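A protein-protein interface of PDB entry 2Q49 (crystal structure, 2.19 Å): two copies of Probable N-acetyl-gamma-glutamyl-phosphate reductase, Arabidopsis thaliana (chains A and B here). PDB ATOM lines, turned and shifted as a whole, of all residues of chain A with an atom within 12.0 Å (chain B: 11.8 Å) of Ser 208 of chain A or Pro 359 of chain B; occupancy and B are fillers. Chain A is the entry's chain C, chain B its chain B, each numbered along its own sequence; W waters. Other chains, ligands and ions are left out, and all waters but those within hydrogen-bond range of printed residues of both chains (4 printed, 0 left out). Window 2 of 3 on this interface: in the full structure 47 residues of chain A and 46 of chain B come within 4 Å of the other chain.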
ATOM      1  N   VAL A 194     -17.468 -36.160  23.748  1.00  0.00           N
ATOM      2  CA  VAL A 194     -16.459 -35.596  22.863  1.00  0.00           C
ATOM      3  C   VAL A 194     -15.579 -36.637  22.145  1.00  0.00           C
ATOM      4  O   VAL A 194     -14.763 -36.275  21.298  1.00  0.00           O
ATOM      5  CB  VAL A 194     -15.605 -34.550  23.641  1.00  0.00           C
ATOM      6  CG1 VAL A 194     -14.805 -35.226  24.741  1.00  0.00           C
ATOM      7  CG2 VAL A 194     -14.707 -33.764  22.676  1.00  0.00           C
ATOM      8  N   LYS A 202      -6.931 -31.183  18.106  1.00  0.00           N
ATOM      9  CA  LYS A 202      -7.603 -29.900  18.013  1.00  0.00           C
ATOM     10  C   LYS A 202      -7.647 -29.175  19.365  1.00  0.00           C
ATOM     11  O   LYS A 202      -7.979 -29.761  20.402  1.00  0.00           O
ATOM     12  CB  LYS A 202      -9.013 -30.106  17.459  1.00  0.00           C
ATOM     13  CG  LYS A 202      -9.010 -30.541  15.991  1.00  0.00           C
ATOM     14  CD  LYS A 202     -10.407 -30.831  15.442  1.00  0.00           C
ATOM     15  CE  LYS A 202     -10.971 -32.162  15.948  1.00  0.00           C
ATOM     16  NZ  LYS A 202     -12.382 -32.403  15.519  1.00  0.00           N
ATOM     17  N   GLU A 203      -7.302 -27.891  19.349  1.00  0.00           N
ATOM     18  CA  GLU A 203      -7.296 -27.091  20.570  1.00  0.00           C
ATOM     19  C   GLU A 203      -8.644 -27.225  21.274  1.00  0.00           C
ATOM     20  O   GLU A 203      -8.718 -27.511  22.475  1.00  0.00           O
ATOM     21  CB  GLU A 203      -7.056 -25.618  20.231  1.00  0.00           C
ATOM     22  CG  GLU A 203      -6.779 -24.745  21.429  1.00  0.00           C
ATOM     23  CD  GLU A 203      -6.692 -23.266  21.070  1.00  0.00           C
ATOM     24  OE1 GLU A 203      -7.748 -22.638  20.854  1.00  0.00           O
ATOM     25  OE2 GLU A 203      -5.566 -22.735  20.997  1.00  0.00           O
ATOM     26  N   ALA A 204      -9.701 -27.024  20.496  1.00  0.00           N
ATOM     27  CA  ALA A 204     -11.059 -27.075  20.991  1.00  0.00           C
ATOM     28  C   ALA A 204     -11.414 -28.315  21.802  1.00  0.00           C
ATOM     29  O   ALA A 204     -12.214 -28.239  22.730  1.00  0.00           O
ATOM     30  CB  ALA A 204     -12.014 -26.935  19.828  1.00  0.00           C
ATOM     31  N   ASN A 205     -10.811 -29.452  21.473  1.00  0.00           N
ATOM     32  CA  ASN A 205     -11.126 -30.694  22.172  1.00  0.00           C
ATOM     33  C   ASN A 205     -10.202 -31.117  23.297  1.00  0.00           C
ATOM     34  O   ASN A 205     -10.277 -32.261  23.761  1.00  0.00           O
ATOM     35  CB  ASN A 205     -11.269 -31.822  21.159  1.00  0.00           C
ATOM     36  CG  ASN A 205     -12.361 -31.540  20.153  1.00  0.00           C
ATOM     37  OD1 ASN A 205     -13.412 -31.011  20.515  1.00  0.00           O
ATOM     38  ND2 ASN A 205     -12.125 -31.886  18.883  1.00  0.00           N
ATOM     39  N   LEU A 206      -9.329 -30.209  23.727  1.00  0.00           N
ATOM     40  CA  LEU A 206      -8.424 -30.485  24.834  1.00  0.00           C
ATOM     41  C   LEU A 206      -9.256 -30.673  26.116  1.00  0.00           C
ATOM     42  O   LEU A 206     -10.379 -30.158  26.224  1.00  0.00           O
ATOM     43  CB  LEU A 206      -7.456 -29.314  25.033  1.00  0.00           C
ATOM     44  CG  LEU A 206      -6.311 -29.169  24.014  1.00  0.00           C
ATOM     45  CD1 LEU A 206      -5.490 -27.877  24.275  1.00  0.00           C
ATOM     46  CD2 LEU A 206      -5.428 -30.413  24.104  1.00  0.00           C
ATOM     47  N   TYR A 207      -8.712 -31.400  27.090  1.00  0.00           N
ATOM     48  CA  TYR A 207      -9.438 -31.604  28.340  1.00  0.00           C
ATOM     49  C   TYR A 207      -9.726 -30.263  29.039  1.00  0.00           C
ATOM     50  O   TYR A 207     -10.839 -30.032  29.513  1.00  0.00           O
ATOM     51  CB  TYR A 207      -8.657 -32.541  29.291  1.00  0.00           C
ATOM     52  CG  TYR A 207      -9.442 -32.883  30.547  1.00  0.00           C
ATOM     53  CD1 TYR A 207      -9.357 -32.086  31.686  1.00  0.00           C
ATOM     54  CD2 TYR A 207     -10.357 -33.938  30.547  1.00  0.00           C
ATOM     55  CE1 TYR A 207     -10.170 -32.318  32.798  1.00  0.00           C
ATOM     56  CE2 TYR A 207     -11.188 -34.189  31.645  1.00  0.00           C
ATOM     57  CZ  TYR A 207     -11.093 -33.368  32.767  1.00  0.00           C
ATOM     58  OH  TYR A 207     -11.949 -33.550  33.832  1.00  0.00           O
ATOM     59  N   SER A 208      -8.726 -29.387  29.099  1.00  0.00           N
ATOM     60  CA  SER A 208      -8.882 -28.099  29.746  1.00  0.00           C
ATOM     61  C   SER A 208      -9.925 -27.202  29.078  1.00  0.00           C
ATOM     62  O   SER A 208     -10.500 -26.313  29.736  1.00  0.00           O
ATOM     63  CB  SER A 208      -7.548 -27.350  29.795  1.00  0.00           C
ATOM     64  OG  SER A 208      -6.535 -28.085  30.458  1.00  0.00           O
ATOM     65  N   GLU A 209     -10.159 -27.402  27.781  1.00  0.00           N
ATOM     66  CA  GLU A 209     -11.138 -26.588  27.059  1.00  0.00           C
ATOM     67  C   GLU A 209     -12.528 -27.215  27.100  1.00  0.00           C
ATOM     68  O   GLU A 209     -13.530 -26.510  27.031  1.00  0.00           O
ATOM     69  CB  GLU A 209     -10.749 -26.423  25.569  1.00  0.00           C
ATOM     70  CG  GLU A 209      -9.337 -25.848  25.253  1.00  0.00           C
ATOM     71  CD  GLU A 209      -9.193 -24.368  25.537  1.00  0.00           C
ATOM     72  OE1 GLU A 209     -10.052 -23.580  25.094  1.00  0.00           O
ATOM     73  OE2 GLU A 209      -8.198 -23.984  26.189  1.00  0.00           O
ATOM     74  N   ILE A 210     -12.591 -28.544  27.190  1.00  0.00           N
ATOM     75  CA  ILE A 210     -13.876 -29.241  27.172  1.00  0.00           C
ATOM     76  C   ILE A 210     -14.509 -29.454  28.533  1.00  0.00           C
ATOM     77  O   ILE A 210     -15.701 -29.245  28.719  1.00  0.00           O
ATOM     78  CB  ILE A 210     -13.727 -30.636  26.509  1.00  0.00           C
ATOM     79  CG1 ILE A 210     -13.443 -30.469  25.005  1.00  0.00           C
ATOM     80  CG2 ILE A 210     -14.956 -31.538  26.836  1.00  0.00           C
ATOM     81  CD1 ILE A 210     -14.609 -29.956  24.181  1.00  0.00           C
ATOM     82  N   ALA A 211     -13.696 -29.883  29.480  1.00  0.00           N
ATOM     83  CA  ALA A 211     -14.192 -30.202  30.804  1.00  0.00           C
ATOM     84  C   ALA A 211     -15.005 -29.133  31.506  1.00  0.00           C
ATOM     85  O   ALA A 211     -14.721 -27.930  31.392  1.00  0.00           O
ATOM     86  CB  ALA A 211     -13.042 -30.646  31.691  1.00  0.00           C
ATOM     87  N   GLU A 212     -16.033 -29.611  32.219  1.00  0.00           N
ATOM     88  CA  GLU A 212     -16.920 -28.778  33.019  1.00  0.00           C
ATOM     89  C   GLU A 212     -17.691 -27.735  32.243  1.00  0.00           C
ATOM     90  O   GLU A 212     -17.804 -26.586  32.674  1.00  0.00           O
ATOM     91  CB  GLU A 212     -16.120 -28.105  34.143  1.00  0.00           C
ATOM     92  CG  GLU A 212     -15.606 -29.080  35.198  1.00  0.00           C
ATOM     93  CD  GLU A 212     -16.735 -29.765  35.987  1.00  0.00           C
ATOM     94  OE1 GLU A 212     -17.591 -29.031  36.530  1.00  0.00           O
ATOM     95  OE2 GLU A 212     -16.756 -31.025  36.071  1.00  0.00           O
ATOM     96  N   GLY A 213     -18.235 -28.148  31.107  1.00  0.00           N
ATOM     97  CA  GLY A 213     -19.019 -27.255  30.292  1.00  0.00           C
ATOM     98  C   GLY A 213     -19.519 -27.965  29.053  1.00  0.00           C
ATOM     99  O   GLY A 213     -18.866 -28.878  28.536  1.00  0.00           O
ATOM    100  N   ILE A 214     -20.687 -27.558  28.577  1.00  0.00           N
ATOM    101  CA  ILE A 214     -21.249 -28.132  27.365  1.00  0.00           C
ATOM    102  C   ILE A 214     -21.317 -27.062  26.276  1.00  0.00           C
ATOM    103  O   ILE A 214     -21.187 -25.867  26.553  1.00  0.00           O
ATOM    104  CB  ILE A 214     -22.701 -28.665  27.569  1.00  0.00           C
ATOM    105  CG1 ILE A 214     -23.653 -27.513  27.931  1.00  0.00           C
ATOM    106  CG2 ILE A 214     -22.719 -29.752  28.604  1.00  0.00           C
ATOM    107  CD1 ILE A 214     -25.134 -27.877  27.717  1.00  0.00           C
ATOM    108  N   SER A 215     -21.538 -27.500  25.044  1.00  0.00           N
ATOM    109  CA  SER A 215     -21.667 -26.570  23.941  1.00  0.00           C
ATOM    110  C   SER A 215     -22.552 -27.071  22.795  1.00  0.00           C
ATOM    111  O   SER A 215     -22.701 -28.279  22.575  1.00  0.00           O
ATOM    112  CB  SER A 215     -20.294 -26.206  23.379  1.00  0.00           C
ATOM    113  OG  SER A 215     -20.447 -25.312  22.301  1.00  0.00           O
ATOM    114  N   LEU A 248     -22.252 -30.720  22.456  1.00  0.00           N
ATOM    115  CA  LEU A 248     -21.065 -31.439  22.914  1.00  0.00           C
ATOM    116  C   LEU A 248     -21.026 -31.504  24.433  1.00  0.00           C
ATOM    117  O   LEU A 248     -21.015 -30.465  25.092  1.00  0.00           O
ATOM    118  CB  LEU A 248     -19.811 -30.730  22.403  1.00  0.00           C
ATOM    119  CG  LEU A 248     -18.464 -31.452  22.489  1.00  0.00           C
ATOM    120  CD1 LEU A 248     -18.512 -32.706  21.627  1.00  0.00           C
ATOM    121  CD2 LEU A 248     -17.370 -30.525  21.985  1.00  0.00           C
ATOM    122  N   MET A 249     -20.998 -32.734  24.961  1.00  0.00           N
ATOM    123  CA  MET A 249     -20.966 -33.015  26.391  1.00  0.00           C
ATOM    124  C   MET A 249     -19.554 -33.240  26.924  1.00  0.00           C
ATOM    125  O   MET A 249     -18.727 -33.876  26.260  1.00  0.00           O
ATOM    126  CB  MET A 249     -21.792 -34.276  26.701  1.00  0.00           C
ATOM    127  CG  MET A 249     -23.249 -34.206  26.241  1.00  0.00           C
ATOM    128  SD  MET A 249     -24.157 -32.974  27.217  1.00  0.00           S
ATOM    129  CE  MET A 249     -24.092 -31.529  26.077  1.00  0.00           C
ATOM    130  N   PRO A 250     -19.263 -32.749  28.152  1.00  0.00           N
ATOM    131  CA  PRO A 250     -17.934 -32.940  28.729  1.00  0.00           C
ATOM    132  C   PRO A 250     -17.817 -34.372  29.245  1.00  0.00           C
ATOM    133  O   PRO A 250     -17.651 -34.615  30.442  1.00  0.00           O
ATOM    134  CB  PRO A 250     -17.896 -31.903  29.855  1.00  0.00           C
ATOM    135  CG  PRO A 250     -19.295 -31.946  30.350  1.00  0.00           C
ATOM    136  CD  PRO A 250     -20.140 -32.027  29.098  1.00  0.00           C
ATOM    137  N   MET A 251     -17.941 -35.320  28.328  1.00  0.00           N
ATOM    138  CA  MET A 251     -17.834 -36.735  28.661  1.00  0.00           C
ATOM    139  C   MET A 251     -17.305 -37.453  27.426  1.00  0.00           C
ATOM    140  O   MET A 251     -17.371 -36.922  26.325  1.00  0.00           O
ATOM    141  CB  MET A 251     -19.201 -37.306  29.060  1.00  0.00           C
ATOM    142  CG  MET A 251     -20.232 -37.285  27.929  1.00  0.00           C
ATOM    143  SD  MET A 251     -21.898 -37.565  28.537  1.00  0.00           S
ATOM    144  CE  MET A 251     -22.797 -37.904  27.033  1.00  0.00           C
ATOM    145  N   ILE A 252     -16.796 -38.668  27.609  1.00  0.00           N
ATOM    146  CA  ILE A 252     -16.232 -39.412  26.488  1.00  0.00           C
ATOM    147  C   ILE A 252     -17.279 -40.045  25.592  1.00  0.00           C
ATOM    148  O   ILE A 252     -17.431 -39.674  24.416  1.00  0.00           O
ATOM    149  CB  ILE A 252     -15.269 -40.531  26.976  1.00  0.00           C
ATOM    150  CG1 ILE A 252     -14.177 -39.950  27.876  1.00  0.00           C
ATOM    151  CG2 ILE A 252     -14.605 -41.217  25.768  1.00  0.00           C
ATOM    152  CD1 ILE A 252     -13.241 -41.019  28.433  1.00  0.00           C
ATOM    153  N   MET B 251     -20.911 -32.228  35.193  1.00  0.00           N
ATOM    154  CA  MET B 251     -20.067 -31.067  35.509  1.00  0.00           C
ATOM    155  C   MET B 251     -20.719 -30.409  36.744  1.00  0.00           C
ATOM    156  O   MET B 251     -21.925 -30.567  36.963  1.00  0.00           O
ATOM    157  CB  MET B 251     -20.052 -30.072  34.338  1.00  0.00           C
ATOM    158  CG  MET B 251     -21.435 -29.541  33.983  1.00  0.00           C
ATOM    159  SD  MET B 251     -21.479 -28.558  32.488  1.00  0.00           S
ATOM    160  CE  MET B 251     -22.459 -27.064  33.041  1.00  0.00           C
ATOM    161  N   ILE B 252     -19.943 -29.678  37.534  1.00  0.00           N
ATOM    162  CA  ILE B 252     -20.483 -29.055  38.736  1.00  0.00           C
ATOM    163  C   ILE B 252     -21.265 -27.758  38.518  1.00  0.00           C
ATOM    164  O   ILE B 252     -22.463 -27.706  38.804  1.00  0.00           O
ATOM    165  CB  ILE B 252     -19.379 -28.801  39.775  1.00  0.00           C
ATOM    166  CG1 ILE B 252     -18.612 -30.100  40.032  1.00  0.00           C
ATOM    167  CG2 ILE B 252     -20.005 -28.299  41.087  1.00  0.00           C
ATOM    168  CD1 ILE B 252     -17.492 -29.964  41.050  1.00  0.00           C
ATOM    169  N   ARG B 253     -20.587 -26.721  38.016  1.00  0.00           N
ATOM    170  CA  ARG B 253     -21.229 -25.432  37.740  1.00  0.00           C
ATOM    171  C   ARG B 253     -21.545 -25.301  36.266  1.00  0.00           C
ATOM    172  O   ARG B 253     -21.048 -26.088  35.447  1.00  0.00           O
ATOM    173  CB  ARG B 253     -20.308 -24.277  38.096  1.00  0.00           C
ATOM    174  CG  ARG B 253     -19.981 -24.163  39.534  1.00  0.00           C
ATOM    175  CD  ARG B 253     -18.835 -23.193  39.748  1.00  0.00           C
ATOM    176  NE  ARG B 253     -18.590 -22.981  41.172  1.00  0.00           N
ATOM    177  CZ  ARG B 253     -19.194 -22.050  41.906  1.00  0.00           C
ATOM    178  NH1 ARG B 253     -20.079 -21.225  41.340  1.00  0.00           N
ATOM    179  NH2 ARG B 253     -18.921 -21.948  43.205  1.00  0.00           N
ATOM    180  N   GLY B 254     -22.343 -24.284  35.933  1.00  0.00           N
ATOM    181  CA  GLY B 254     -22.693 -24.022  34.545  1.00  0.00           C
ATOM    182  C   GLY B 254     -24.128 -24.302  34.170  1.00  0.00           C
ATOM    183  O   GLY B 254     -24.741 -25.228  34.707  1.00  0.00           O
ATOM    184  N   ARG B 296     -20.653 -20.609  25.389  1.00  0.00           N
ATOM    185  CA  ARG B 296     -20.110 -21.768  26.104  1.00  0.00           C
ATOM    186  C   ARG B 296     -20.194 -21.510  27.605  1.00  0.00           C
ATOM    187  O   ARG B 296     -19.592 -20.552  28.075  1.00  0.00           O
ATOM    188  CB  ARG B 296     -18.638 -21.988  25.720  1.00  0.00           C
ATOM    189  CG  ARG B 296     -18.457 -22.776  24.436  1.00  0.00           C
ATOM    190  CD  ARG B 296     -17.022 -22.721  23.904  1.00  0.00           C
ATOM    191  NE  ARG B 296     -15.947 -22.901  24.886  1.00  0.00           N
ATOM    192  CZ  ARG B 296     -15.511 -24.076  25.343  1.00  0.00           C
ATOM    193  NH1 ARG B 296     -16.057 -25.215  24.931  1.00  0.00           N
ATOM    194  NH2 ARG B 296     -14.484 -24.117  26.185  1.00  0.00           N
ATOM    195  N   THR B 297     -20.914 -22.353  28.353  1.00  0.00           N
ATOM    196  CA  THR B 297     -21.032 -22.149  29.796  1.00  0.00           C
ATOM    197  C   THR B 297     -19.642 -21.995  30.419  1.00  0.00           C
ATOM    198  O   THR B 297     -19.477 -21.379  31.484  1.00  0.00           O
ATOM    199  CB  THR B 297     -21.790 -23.317  30.513  1.00  0.00           C
ATOM    200  OG1 THR B 297     -21.059 -24.536  30.365  1.00  0.00           O
ATOM    201  CG2 THR B 297     -23.200 -23.501  29.928  1.00  0.00           C
ATOM    202  N   HIS B 298     -18.642 -22.564  29.745  1.00  0.00           N
ATOM    203  CA  HIS B 298     -17.245 -22.486  30.207  1.00  0.00           C
ATOM    204  C   HIS B 298     -16.860 -21.007  30.307  1.00  0.00           C
ATOM    205  O   HIS B 298     -16.018 -20.621  31.123  1.00  0.00           O
ATOM    206  CB  HIS B 298     -16.260 -23.124  29.197  1.00  0.00           C
ATOM    207  CG  HIS B 298     -16.666 -24.473  28.670  1.00  0.00           C
ATOM    208  ND1 HIS B 298     -17.715 -24.651  27.796  1.00  0.00           N
ATOM    209  CD2 HIS B 298     -16.116 -25.700  28.847  1.00  0.00           C
ATOM    210  CE1 HIS B 298     -17.794 -25.926  27.454  1.00  0.00           C
ATOM    211  NE2 HIS B 298     -16.833 -26.586  28.078  1.00  0.00           N
ATOM    212  N   ASN B 299     -17.475 -20.183  29.464  1.00  0.00           N
ATOM    213  CA  ASN B 299     -17.152 -18.762  29.425  1.00  0.00           C
ATOM    214  C   ASN B 299     -17.818 -17.874  30.468  1.00  0.00           C
ATOM    215  O   ASN B 299     -17.440 -16.710  30.604  1.00  0.00           O
ATOM    216  CB  ASN B 299     -17.422 -18.218  28.024  1.00  0.00           C
ATOM    217  CG  ASN B 299     -16.540 -18.886  26.971  1.00  0.00           C
ATOM    218  OD1 ASN B 299     -15.391 -19.232  27.263  1.00  0.00           O
ATOM    219  ND2 ASN B 299     -17.061 -19.067  25.755  1.00  0.00           N
ATOM    220  N   VAL B 300     -18.799 -18.416  31.188  1.00  0.00           N
ATOM    221  CA  VAL B 300     -19.505 -17.679  32.234  1.00  0.00           C
ATOM    222  C   VAL B 300     -19.543 -18.518  33.522  1.00  0.00           C
ATOM    223  O   VAL B 300     -20.540 -18.517  34.253  1.00  0.00           O
ATOM    224  CB  VAL B 300     -20.965 -17.350  31.822  1.00  0.00           C
ATOM    225  CG1 VAL B 300     -20.966 -16.558  30.529  1.00  0.00           C
ATOM    226  CG2 VAL B 300     -21.817 -18.639  31.688  1.00  0.00           C
ATOM    227  N   ARG B 301     -18.433 -19.210  33.784  1.00  0.00           N
ATOM    228  CA  ARG B 301     -18.257 -20.106  34.925  1.00  0.00           C
ATOM    229  C   ARG B 301     -17.567 -19.422  36.095  1.00  0.00           C
ATOM    230  O   ARG B 301     -16.383 -19.079  36.022  1.00  0.00           O
ATOM    231  CB  ARG B 301     -17.429 -21.327  34.476  1.00  0.00           C
ATOM    232  CG  ARG B 301     -17.550 -22.557  35.339  1.00  0.00           C
ATOM    233  CD  ARG B 301     -16.913 -23.774  34.676  1.00  0.00           C
ATOM    234  NE  ARG B 301     -15.497 -23.619  34.337  1.00  0.00           N
ATOM    235  CZ  ARG B 301     -14.934 -24.219  33.285  1.00  0.00           C
ATOM    236  NH1 ARG B 301     -15.674 -24.986  32.493  1.00  0.00           N
ATOM    237  NH2 ARG B 301     -13.641 -24.082  33.027  1.00  0.00           N
ATOM    238  N   GLY B 302     -18.308 -19.234  37.179  1.00  0.00           N
ATOM    239  CA  GLY B 302     -17.732 -18.592  38.342  1.00  0.00           C
ATOM    240  C   GLY B 302     -17.833 -17.073  38.297  1.00  0.00           C
ATOM    241  O   GLY B 302     -17.212 -16.383  39.091  1.00  0.00           O
ATOM    242  N   SER B 303     -18.618 -16.557  37.359  1.00  0.00           N
ATOM    243  CA  SER B 303     -18.806 -15.118  37.209  1.00  0.00           C
ATOM    244  C   SER B 303     -20.296 -14.848  37.199  1.00  0.00           C
ATOM    245  O   SER B 303     -21.112 -15.753  37.015  1.00  0.00           O
ATOM    246  CB  SER B 303     -18.231 -14.627  35.879  1.00  0.00           C
ATOM    247  OG  SER B 303     -19.012 -15.137  34.801  1.00  0.00           O
ATOM    248  N   ASP B 326     -23.965 -19.259  34.677  1.00  0.00           N
ATOM    249  CA  ASP B 326     -23.420 -20.129  35.710  1.00  0.00           C
ATOM    250  C   ASP B 326     -24.647 -20.261  36.645  1.00  0.00           C
ATOM    251  O   ASP B 326     -25.016 -19.291  37.293  1.00  0.00           O
ATOM    252  CB  ASP B 326     -22.277 -19.454  36.480  1.00  0.00           C
ATOM    253  CG  ASP B 326     -21.746 -20.337  37.606  1.00  0.00           C
ATOM    254  OD1 ASP B 326     -22.594 -20.979  38.268  1.00  0.00           O
ATOM    255  OD2 ASP B 326     -20.508 -20.389  37.823  1.00  0.00           O
ATOM    256  N   GLN B 355     -14.174 -12.194  37.358  1.00  0.00           N
ATOM    257  CA  GLN B 355     -13.904 -12.682  35.997  1.00  0.00           C
ATOM    258  C   GLN B 355     -14.160 -14.192  35.923  1.00  0.00           C
ATOM    259  O   GLN B 355     -13.937 -14.905  36.898  1.00  0.00           O
ATOM    260  CB  GLN B 355     -12.456 -12.379  35.590  1.00  0.00           C
ATOM    261  CG  GLN B 355     -12.241 -10.965  35.091  1.00  0.00           C
ATOM    262  CD  GLN B 355     -13.031 -10.686  33.831  1.00  0.00           C
ATOM    263  OE1 GLN B 355     -12.874 -11.367  32.802  1.00  0.00           O
ATOM    264  NE2 GLN B 355     -13.887  -9.678  33.899  1.00  0.00           N
ATOM    265  N   PRO B 356     -14.607 -14.704  34.757  1.00  0.00           N
ATOM    266  CA  PRO B 356     -14.870 -16.153  34.678  1.00  0.00           C
ATOM    267  C   PRO B 356     -13.638 -17.008  34.968  1.00  0.00           C
ATOM    268  O   PRO B 356     -12.506 -16.599  34.682  1.00  0.00           O
ATOM    269  CB  PRO B 356     -15.385 -16.344  33.253  1.00  0.00           C
ATOM    270  CG  PRO B 356     -15.984 -14.995  32.926  1.00  0.00           C
ATOM    271  CD  PRO B 356     -14.947 -14.043  33.484  1.00  0.00           C
ATOM    272  N   LEU B 357     -13.861 -18.185  35.543  1.00  0.00           N
ATOM    273  CA  LEU B 357     -12.763 -19.084  35.835  1.00  0.00           C
ATOM    274  C   LEU B 357     -12.556 -20.008  34.629  1.00  0.00           C
ATOM    275  O   LEU B 357     -13.314 -20.953  34.421  1.00  0.00           O
ATOM    276  CB  LEU B 357     -13.046 -19.923  37.091  1.00  0.00           C
ATOM    277  CG  LEU B 357     -11.774 -20.625  37.596  1.00  0.00           C
ATOM    278  CD1 LEU B 357     -10.722 -19.557  37.971  1.00  0.00           C
ATOM    279  CD2 LEU B 357     -12.085 -21.522  38.782  1.00  0.00           C
ATOM    280  N   PHE B 358     -11.541 -19.707  33.824  1.00  0.00           N
ATOM    281  CA  PHE B 358     -11.236 -20.503  32.648  1.00  0.00           C
ATOM    282  C   PHE B 358      -9.721 -20.526  32.436  1.00  0.00           C
ATOM    283  O   PHE B 358      -9.062 -19.495  32.480  1.00  0.00           O
ATOM    284  CB  PHE B 358     -11.959 -19.948  31.412  1.00  0.00           C
ATOM    285  CG  PHE B 358     -11.687 -20.730  30.143  1.00  0.00           C
ATOM    286  CD1 PHE B 358     -10.482 -20.577  29.450  1.00  0.00           C
ATOM    287  CD2 PHE B 358     -12.612 -21.650  29.667  1.00  0.00           C
ATOM    288  CE1 PHE B 358     -10.203 -21.329  28.298  1.00  0.00           C
ATOM    289  CE2 PHE B 358     -12.339 -22.417  28.509  1.00  0.00           C
ATOM    290  CZ  PHE B 358     -11.133 -22.251  27.831  1.00  0.00           C
ATOM    291  N   PRO B 359      -9.153 -21.721  32.207  1.00  0.00           N
ATOM    292  CA  PRO B 359      -9.929 -22.969  32.189  1.00  0.00           C
ATOM    293  C   PRO B 359     -10.323 -23.398  33.603  1.00  0.00           C
ATOM    294  O   PRO B 359      -9.790 -22.806  34.552  1.00  0.00           O
ATOM    295  CB  PRO B 359      -8.973 -23.943  31.506  1.00  0.00           C
ATOM    296  CG  PRO B 359      -7.626 -23.480  31.983  1.00  0.00           C
ATOM    297  CD  PRO B 359      -7.724 -21.971  31.938  1.00  0.00           C
ATOM    298  OXT PRO B 359     -11.155 -24.301  33.761  1.00  0.00           O
HETATM  299  O   HOH W   1     -15.176 -26.717  22.119  1.00  0.00           O
HETATM  300  O   HOH W   2     -13.142 -25.997  30.525  1.00  0.00           O
HETATM  301  O   HOH W   3     -20.033 -24.726  32.564  1.00  0.00           O
HETATM  302  O   HOH W   4     -18.293 -26.660  36.592  1.00  0.00           O
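Water W2 lies within hydrogen-bond range of O of Ala 211 of chain A (2.6 Å), O of Ser 208 of chain A (2.8 Å) and NH2 of Arg 301 of chain B (3.2 Å).
Water W1 lies within hydrogen-bond range of NH1 of Arg 296 of chain B (3.3 Å) and O of Ala 204 of chain A (3.4 Å).
Positions printed for both chains: 251 and 252.
Of the 16 pairs that touch across the chains among the printed residues, none has its exchanged pair printed and touching as well.
NH2 of Arg 301 of chain B is in salt-bridge range of OXT of Pro 359 of chain B (2.6 Å).
The backbone NH of Leu 357 of chain B lies within hydrogen-bond range of the backbone carbonyl oxygen of Arg 301 of chain B, 2.7 Å away.
The backbone carbonyl oxygen (O) of Ser 215 of chain A sits at hydrogen-bond distance from the backbone NH (N) of Leu 248 of chain A (2.5 Å).
A ring nitrogen (ND1) of His 298 of chain B lies close to the guanidinium group (NH1) of Arg 296 of chain B (3.4 Å).
Of the printed residues of chain B, Ser 208 of chain A touches Pro 359 (3.3 Å).
Of chain A, only Ser 208 (3.3 Å) comes within 4 Å of Pro 359 of chain B.
No residue of chain B comes within 4 Å of Tyr 207 of chain A.
Of chain B, only His 298 (3.0 Å) comes within 4 Å of Ile 210 of chain A.
Of chain B, only His 298 (3.7 Å) and Arg 301 (3.3 Å) come within 4 Å of Ala 211 of chain A.
Of chain A, only Glu 209 (3.2 Å) comes within 4 Å of Phe 358 of chain B.
Printed residues of chain A within 4 Å of Thr 297 of chain B: Gly 213 and Ile 214.
Of the printed residues of chain B, Gly 213 of chain A touches Met 251, Thr 297 and His 298.
Gly 254 of chain B touches none of the printed residues of chain A.
Met 249 of chain A touches none of the printed residues of chain B.
The nearest printed residue of chain A that does not touch Arg 301 of chain B is Gly 213 of chain A (4.3 Å).
Of the 20 printed residues of chain A, 8 touch a printed residue of chain B.
Hydrophobic or aromatic side chains of chain B that line the printed part of chain A: Met 251, Ile 252, His 298, Phe 358 and Pro 359.
The backbone carbonyl oxygen (O) of Ile 210 of chain A is in hydrogen-bond range of a ring nitrogen (NE2) of His 298 of chain B (3.0 Å).
NH1 of Arg 301 of chain B is in hydrogen-bond range of O of Ala 211 of chain A.
SD of Met 251 of chain B lies close to N of Gly 213 of chain A (3.5 Å).
N of Ile 252 of chain B is in hydrogen-bond range of OE1 of Glu 212 of chain A (2.6 Å).
The guanidinium group of Arg 296 of chain B lies within hydrogen-bond range of the backbone carbonyl oxygen of Glu 209 of chain A (2.7 Å).
The backbone carbonyl oxygen (O) of Glu 212 of chain A sits at hydrogen-bond distance from the guanidinium group (NH1) of Arg 301 of chain B.
The backbone carbonyl oxygen of Gly 213 of chain A lies within hydrogen-bond range of a ring nitrogen (NE2) of His 298 of chain B (3.1 Å).
A ring nitrogen (NE2) of His 298 of chain B sits close to the backbone carbonyl oxygen of Glu 209 of chain A (3.5 Å).
Glu 209 of chain A touches Phe 358 of chain B.
Ala 211 of chain A touches His 298 of chain B (O to CD2, 3.7 Å).
CA of Met 251 of chain B touches OE2 of Glu 212 of chain A, at 3.4 Å.
Gly 213 of chain A touches Thr 297 of chain B (CA to OG1, 3.4 Å).
N of Ile 214 of chain A touches OG1 of Thr 297 of chain B (3.5 Å).
CE1 of His 298 of chain B touches N of Ile 214 of chain A, at 3.5 Å.
Arg 296 of chain B touches Ser 215 of chain A (CG to OG, 3.9 Å).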
